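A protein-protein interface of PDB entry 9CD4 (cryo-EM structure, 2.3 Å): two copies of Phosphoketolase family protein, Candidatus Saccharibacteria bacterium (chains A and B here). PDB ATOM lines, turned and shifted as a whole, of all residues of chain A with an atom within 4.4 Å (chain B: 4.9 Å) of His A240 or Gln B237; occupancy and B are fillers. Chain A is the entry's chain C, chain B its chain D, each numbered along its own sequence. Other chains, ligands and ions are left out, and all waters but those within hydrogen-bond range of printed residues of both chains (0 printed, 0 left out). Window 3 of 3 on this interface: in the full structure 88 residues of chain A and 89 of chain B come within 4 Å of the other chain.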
ATOM      1  N   ILE A 236     -16.862  13.339  -4.818  1.00  0.00           N
ATOM      2  CA  ILE A 236     -15.938  14.106  -5.650  1.00  0.00           C
ATOM      3  C   ILE A 236     -15.124  15.066  -4.793  1.00  0.00           C
ATOM      4  O   ILE A 236     -13.897  15.147  -4.921  1.00  0.00           O
ATOM      5  CB  ILE A 236     -16.700  14.849  -6.763  1.00  0.00           C
ATOM      6  CG1 ILE A 236     -17.171  13.871  -7.842  1.00  0.00           C
ATOM      7  CG2 ILE A 236     -15.836  15.939  -7.381  1.00  0.00           C
ATOM      8  CD1 ILE A 236     -16.058  13.093  -8.494  1.00  0.00           C
ATOM      9  N   GLN A 237     -15.791  15.793  -3.888  1.00  0.00           N
ATOM     10  CA  GLN A 237     -15.059  16.708  -3.014  1.00  0.00           C
ATOM     11  C   GLN A 237     -14.113  15.972  -2.074  1.00  0.00           C
ATOM     12  O   GLN A 237     -12.990  16.433  -1.838  1.00  0.00           O
ATOM     13  CB  GLN A 237     -16.019  17.585  -2.215  1.00  0.00           C
ATOM     14  CG  GLN A 237     -16.178  18.978  -2.785  1.00  0.00           C
ATOM     15  CD  GLN A 237     -17.235  19.780  -2.067  1.00  0.00           C
ATOM     16  OE1 GLN A 237     -17.796  20.723  -2.621  1.00  0.00           O
ATOM     17  NE2 GLN A 237     -17.521  19.404  -0.829  1.00  0.00           N
ATOM     18  N   PHE A 238     -14.540  14.832  -1.524  1.00  0.00           N
ATOM     19  CA  PHE A 238     -13.685  14.105  -0.591  1.00  0.00           C
ATOM     20  C   PHE A 238     -12.440  13.561  -1.279  1.00  0.00           C
ATOM     21  O   PHE A 238     -11.338  13.641  -0.726  1.00  0.00           O
ATOM     22  CB  PHE A 238     -14.467  12.973   0.073  1.00  0.00           C
ATOM     23  CG  PHE A 238     -13.659  12.183   1.063  1.00  0.00           C
ATOM     24  CD1 PHE A 238     -13.446  12.666   2.343  1.00  0.00           C
ATOM     25  CD2 PHE A 238     -13.116  10.955   0.718  1.00  0.00           C
ATOM     26  CE1 PHE A 238     -12.704  11.944   3.258  1.00  0.00           C
ATOM     27  CE2 PHE A 238     -12.373  10.230   1.628  1.00  0.00           C
ATOM     28  CZ  PHE A 238     -12.168  10.725   2.900  1.00  0.00           C
ATOM     29  N   PHE A 239     -12.587  13.010  -2.483  1.00  0.00           N
ATOM     30  CA  PHE A 239     -11.442  12.433  -3.172  1.00  0.00           C
ATOM     31  C   PHE A 239     -10.627  13.456  -3.954  1.00  0.00           C
ATOM     32  O   PHE A 239      -9.504  13.142  -4.364  1.00  0.00           O
ATOM     33  CB  PHE A 239     -11.900  11.303  -4.098  1.00  0.00           C
ATOM     34  CG  PHE A 239     -12.248  10.042  -3.367  1.00  0.00           C
ATOM     35  CD1 PHE A 239     -11.274   9.340  -2.676  1.00  0.00           C
ATOM     36  CD2 PHE A 239     -13.547   9.566  -3.351  1.00  0.00           C
ATOM     37  CE1 PHE A 239     -11.589   8.183  -1.994  1.00  0.00           C
ATOM     38  CE2 PHE A 239     -13.867   8.408  -2.669  1.00  0.00           C
ATOM     39  CZ  PHE A 239     -12.886   7.716  -1.991  1.00  0.00           C
ATOM     40  N   HIS A 240     -11.150  14.662  -4.169  1.00  0.00           N
ATOM     41  CA  HIS A 240     -10.342  15.742  -4.714  1.00  0.00           C
ATOM     42  C   HIS A 240      -9.678  16.579  -3.630  1.00  0.00           C
ATOM     43  O   HIS A 240      -8.742  17.327  -3.931  1.00  0.00           O
ATOM     44  CB  HIS A 240     -11.198  16.644  -5.606  1.00  0.00           C
ATOM     45  CG  HIS A 240     -10.402  17.531  -6.510  1.00  0.00           C
ATOM     46  ND1 HIS A 240     -10.312  18.894  -6.326  1.00  0.00           N
ATOM     47  CD2 HIS A 240      -9.660  17.251  -7.608  1.00  0.00           C
ATOM     48  CE1 HIS A 240      -9.548  19.416  -7.268  1.00  0.00           C
ATOM     49  NE2 HIS A 240      -9.141  18.440  -8.061  1.00  0.00           N
ATOM     50  N   GLY A 241     -10.139  16.471  -2.381  1.00  0.00           N
ATOM     51  CA  GLY A 241      -9.449  17.131  -1.288  1.00  0.00           C
ATOM     52  C   GLY A 241      -8.089  16.528  -1.010  1.00  0.00           C
ATOM     53  O   GLY A 241      -7.195  17.211  -0.505  1.00  0.00           O
ATOM     54  N   ALA A 242      -7.915  15.250  -1.328  1.00  0.00           N
ATOM     55  CA  ALA A 242      -6.606  14.619  -1.323  1.00  0.00           C
ATOM     56  C   ALA A 242      -5.976  14.791  -2.704  1.00  0.00           C
ATOM     57  O   ALA A 242      -6.467  15.550  -3.544  1.00  0.00           O
ATOM     58  CB  ALA A 242      -6.726  13.152  -0.915  1.00  0.00           C
ATOM     59  N   TRP A 244      -5.947  13.244  -5.648  1.00  0.00           N
ATOM     60  CA  TRP A 244      -6.503  12.291  -6.596  1.00  0.00           C
ATOM     61  C   TRP A 244      -7.456  13.002  -7.545  1.00  0.00           C
ATOM     62  O   TRP A 244      -8.003  14.064  -7.235  1.00  0.00           O
ATOM     63  CB  TRP A 244      -7.232  11.146  -5.884  1.00  0.00           C
ATOM     64  CG  TRP A 244      -6.362  10.371  -4.952  1.00  0.00           C
ATOM     65  CD1 TRP A 244      -6.269  10.524  -3.602  1.00  0.00           C
ATOM     66  CD2 TRP A 244      -5.446   9.327  -5.302  1.00  0.00           C
ATOM     67  NE1 TRP A 244      -5.358   9.636  -3.086  1.00  0.00           N
ATOM     68  CE2 TRP A 244      -4.838   8.889  -4.109  1.00  0.00           C
ATOM     69  CE3 TRP A 244      -5.082   8.718  -6.506  1.00  0.00           C
ATOM     70  CZ2 TRP A 244      -3.889   7.872  -4.086  1.00  0.00           C
ATOM     71  CZ3 TRP A 244      -4.139   7.708  -6.481  1.00  0.00           C
ATOM     72  CH2 TRP A 244      -3.554   7.295  -5.279  1.00  0.00           C
ATOM     73  N   GLU A 245      -7.645  12.396  -8.714  1.00  0.00           N
ATOM     74  CA  GLU A 245      -8.596  12.873  -9.719  1.00  0.00           C
ATOM     75  C   GLU A 245      -9.638  11.788  -9.947  1.00  0.00           C
ATOM     76  O   GLU A 245      -9.362  10.796 -10.644  1.00  0.00           O
ATOM     77  CB  GLU A 245      -7.883  13.219 -11.025  1.00  0.00           C
ATOM     78  CG  GLU A 245      -8.724  14.024 -11.997  1.00  0.00           C
ATOM     79  CD  GLU A 245      -8.702  15.506 -11.692  1.00  0.00           C
ATOM     80  OE1 GLU A 245      -7.690  15.982 -11.138  1.00  0.00           O
ATOM     81  OE2 GLU A 245      -9.694  16.196 -12.009  1.00  0.00           O
ATOM     82  N   ARG A 285      -1.381  14.620  -9.710  1.00  0.00           N
ATOM     83  CA  ARG A 285      -2.725  14.185  -9.333  1.00  0.00           C
ATOM     84  C   ARG A 285      -3.032  12.899 -10.093  1.00  0.00           C
ATOM     85  O   ARG A 285      -3.417  12.940 -11.265  1.00  0.00           O
ATOM     86  CB  ARG A 285      -3.758  15.269  -9.627  1.00  0.00           C
ATOM     87  CG  ARG A 285      -3.559  16.545  -8.825  1.00  0.00           C
ATOM     88  CD  ARG A 285      -4.867  17.062  -8.257  1.00  0.00           C
ATOM     89  NE  ARG A 285      -5.880  17.236  -9.291  1.00  0.00           N
ATOM     90  CZ  ARG A 285      -6.381  18.408  -9.656  1.00  0.00           C
ATOM     91  NH1 ARG A 285      -5.979  19.537  -9.096  1.00  0.00           N
ATOM     92  NH2 ARG A 285      -7.310  18.447 -10.606  1.00  0.00           N
ATOM     93  N   PHE B 233      -7.762  25.730   0.167  1.00  0.00           N
ATOM     94  CA  PHE B 233      -8.789  25.183  -0.714  1.00  0.00           C
ATOM     95  C   PHE B 233      -8.896  23.667  -0.570  1.00  0.00           C
ATOM     96  O   PHE B 233     -10.003  23.115  -0.489  1.00  0.00           O
ATOM     97  CB  PHE B 233      -8.462  25.583  -2.154  1.00  0.00           C
ATOM     98  CG  PHE B 233      -9.612  25.467  -3.105  1.00  0.00           C
ATOM     99  CD1 PHE B 233      -9.731  24.374  -3.944  1.00  0.00           C
ATOM    100  CD2 PHE B 233     -10.567  26.468  -3.173  1.00  0.00           C
ATOM    101  CE1 PHE B 233     -10.784  24.281  -4.831  1.00  0.00           C
ATOM    102  CE2 PHE B 233     -11.626  26.376  -4.053  1.00  0.00           C
ATOM    103  CZ  PHE B 233     -11.735  25.280  -4.881  1.00  0.00           C
ATOM    104  N   GLU B 234      -7.749  22.984  -0.511  1.00  0.00           N
ATOM    105  CA  GLU B 234      -7.740  21.532  -0.356  1.00  0.00           C
ATOM    106  C   GLU B 234      -8.305  21.110   0.995  1.00  0.00           C
ATOM    107  O   GLU B 234      -9.054  20.131   1.080  1.00  0.00           O
ATOM    108  CB  GLU B 234      -6.319  20.999  -0.526  1.00  0.00           C
ATOM    109  CG  GLU B 234      -5.843  20.925  -1.964  1.00  0.00           C
ATOM    110  CD  GLU B 234      -4.337  20.786  -2.066  1.00  0.00           C
ATOM    111  OE1 GLU B 234      -3.640  21.822  -2.040  1.00  0.00           O
ATOM    112  OE2 GLU B 234      -3.850  19.640  -2.166  1.00  0.00           O
ATOM    113  N   LEU B 235      -7.949  21.832   2.061  1.00  0.00           N
ATOM    114  CA  LEU B 235      -8.484  21.523   3.385  1.00  0.00           C
ATOM    115  C   LEU B 235      -9.989  21.745   3.438  1.00  0.00           C
ATOM    116  O   LEU B 235     -10.723  20.946   4.035  1.00  0.00           O
ATOM    117  CB  LEU B 235      -7.783  22.372   4.445  1.00  0.00           C
ATOM    118  CG  LEU B 235      -6.350  21.995   4.820  1.00  0.00           C
ATOM    119  CD1 LEU B 235      -5.630  23.192   5.413  1.00  0.00           C
ATOM    120  CD2 LEU B 235      -6.339  20.832   5.794  1.00  0.00           C
ATOM    121  N   ILE B 236     -10.464  22.828   2.813  1.00  0.00           N
ATOM    122  CA  ILE B 236     -11.897  23.112   2.778  1.00  0.00           C
ATOM    123  C   ILE B 236     -12.640  21.994   2.060  1.00  0.00           C
ATOM    124  O   ILE B 236     -13.664  21.499   2.545  1.00  0.00           O
ATOM    125  CB  ILE B 236     -12.159  24.479   2.121  1.00  0.00           C
ATOM    126  CG1 ILE B 236     -11.807  25.619   3.079  1.00  0.00           C
ATOM    127  CG2 ILE B 236     -13.609  24.599   1.670  1.00  0.00           C
ATOM    128  CD1 ILE B 236     -12.557  25.579   4.385  1.00  0.00           C
ATOM    129  N   GLN B 237     -12.120  21.558   0.907  1.00  0.00           N
ATOM    130  CA  GLN B 237     -12.758  20.456   0.188  1.00  0.00           C
ATOM    131  C   GLN B 237     -12.728  19.159   0.988  1.00  0.00           C
ATOM    132  O   GLN B 237     -13.734  18.441   1.053  1.00  0.00           O
ATOM    133  CB  GLN B 237     -12.103  20.247  -1.174  1.00  0.00           C
ATOM    134  CG  GLN B 237     -12.914  20.796  -2.326  1.00  0.00           C
ATOM    135  CD  GLN B 237     -12.297  20.469  -3.668  1.00  0.00           C
ATOM    136  OE1 GLN B 237     -11.975  19.318  -3.947  1.00  0.00           O
ATOM    137  NE2 GLN B 237     -12.165  21.471  -4.519  1.00  0.00           N
ATOM    138  N   PHE B 238     -11.588  18.845   1.610  1.00  0.00           N
ATOM    139  CA  PHE B 238     -11.459  17.583   2.329  1.00  0.00           C
ATOM    140  C   PHE B 238     -12.390  17.524   3.531  1.00  0.00           C
ATOM    141  O   PHE B 238     -12.977  16.473   3.814  1.00  0.00           O
ATOM    142  CB  PHE B 238     -10.009  17.368   2.763  1.00  0.00           C
ATOM    143  CG  PHE B 238      -9.778  16.068   3.478  1.00  0.00           C
ATOM    144  CD1 PHE B 238      -9.630  14.890   2.767  1.00  0.00           C
ATOM    145  CD2 PHE B 238      -9.700  16.024   4.860  1.00  0.00           C
ATOM    146  CE1 PHE B 238      -9.418  13.692   3.420  1.00  0.00           C
ATOM    147  CE2 PHE B 238      -9.488  14.829   5.519  1.00  0.00           C
ATOM    148  CZ  PHE B 238      -9.346  13.662   4.797  1.00  0.00           C
ATOM    149  N   PHE B 239     -12.544  18.634   4.251  1.00  0.00           N
ATOM    150  CA  PHE B 239     -13.398  18.624   5.430  1.00  0.00           C
ATOM    151  C   PHE B 239     -14.862  18.910   5.120  1.00  0.00           C
ATOM    152  O   PHE B 239     -15.723  18.595   5.947  1.00  0.00           O
ATOM    153  CB  PHE B 239     -12.869  19.618   6.465  1.00  0.00           C
ATOM    154  CG  PHE B 239     -11.630  19.144   7.162  1.00  0.00           C
ATOM    155  CD1 PHE B 239     -11.663  18.013   7.959  1.00  0.00           C
ATOM    156  CD2 PHE B 239     -10.427  19.808   7.000  1.00  0.00           C
ATOM    157  CE1 PHE B 239     -10.524  17.563   8.596  1.00  0.00           C
ATOM    158  CE2 PHE B 239      -9.284  19.363   7.634  1.00  0.00           C
ATOM    159  CZ  PHE B 239      -9.333  18.239   8.434  1.00  0.00           C
ATOM    160  N   HIS B 240     -15.169  19.487   3.956  1.00  0.00           N
ATOM    161  CA  HIS B 240     -16.559  19.588   3.530  1.00  0.00           C
ATOM    162  C   HIS B 240     -17.068  18.267   2.974  1.00  0.00           C
ATOM    163  O   HIS B 240     -18.251  17.946   3.136  1.00  0.00           O
ATOM    164  CB  HIS B 240     -16.706  20.693   2.484  1.00  0.00           C
ATOM    165  CG  HIS B 240     -18.122  21.112   2.237  1.00  0.00           C
ATOM    166  ND1 HIS B 240     -19.048  20.292   1.630  1.00  0.00           N
ATOM    167  CD2 HIS B 240     -18.765  22.273   2.503  1.00  0.00           C
ATOM    168  CE1 HIS B 240     -20.203  20.927   1.540  1.00  0.00           C
ATOM    169  NE2 HIS B 240     -20.058  22.131   2.061  1.00  0.00           N
ATOM    170  N   GLY B 241     -16.200  17.492   2.320  1.00  0.00           N
ATOM    171  CA  GLY B 241     -16.611  16.207   1.782  1.00  0.00           C
ATOM    172  C   GLY B 241     -16.831  15.142   2.833  1.00  0.00           C
ATOM    173  O   GLY B 241     -17.485  14.134   2.550  1.00  0.00           O
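The side-chain amide nitrogen (NE2) of Gln A237 lies within hydrogen-bond range of a ring nitrogen (ND1) of His B240. OE1 of Gln B237 sits at hydrogen-bond distance from ND1 of His A240, 2.9 Å away.
O of Gln A237 touches O of Gln B237 (3.6 Å). Gln A237 touches Gly B241. CE1 of Phe A238 touches CE1 of Phe B238 (3.7 Å). Gly A241 touches Glu B234 (O to O, 3.8 Å). N of Gly A241 touches OE1 of Gln B237 (3.7 Å). Gly A241 touches Phe B238 (CA to N, 3.99 Å).
Hydrophobic or aromatic side chains of chain B within 4 Å of the printed part of chain A: Phe B238 and His B240. Printed residues of chain A that touch a printed residue of chain B: Gln A237, Phe A238, His A240 and Gly A241.
Of chain B, only Gln B237 (2.9 Å) comes within 4 Å of His A240. Of chain A, only Gln A237, His A240 and Gly A241 come within 4 Å of Gln B237. Of the printed residues of chain B, Gly A241 touches Glu B234 (3.8 Å), Gln B237 (3.7 Å) and Phe B238 (3.99 Å). Printed residues of chain B within 4 Å of Phe A238: Phe B238 (3.7 Å). Ala A242 touches none of the printed residues of chain B. The nearest printed residue of chain A that does not touch Glu B234 is His A240 (5.0 Å).
Gln A237 touches His B240, and with the chains exchanged His A240 touches Gln B237. Gln A237 touches Gly B241, and with the chains exchanged Gly A241 touches Gln B237. Phe A238 touches its own counterpart, Phe B238. Gly A241 touches Phe B238, but with the chains exchanged Phe A238 does not touch Gly B241 (4.1 Å).
A ring nitrogen (NE2) of His A240 sits at hydrogen-bond distance from the guanidinium group of Arg A285 (3.1 Å).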
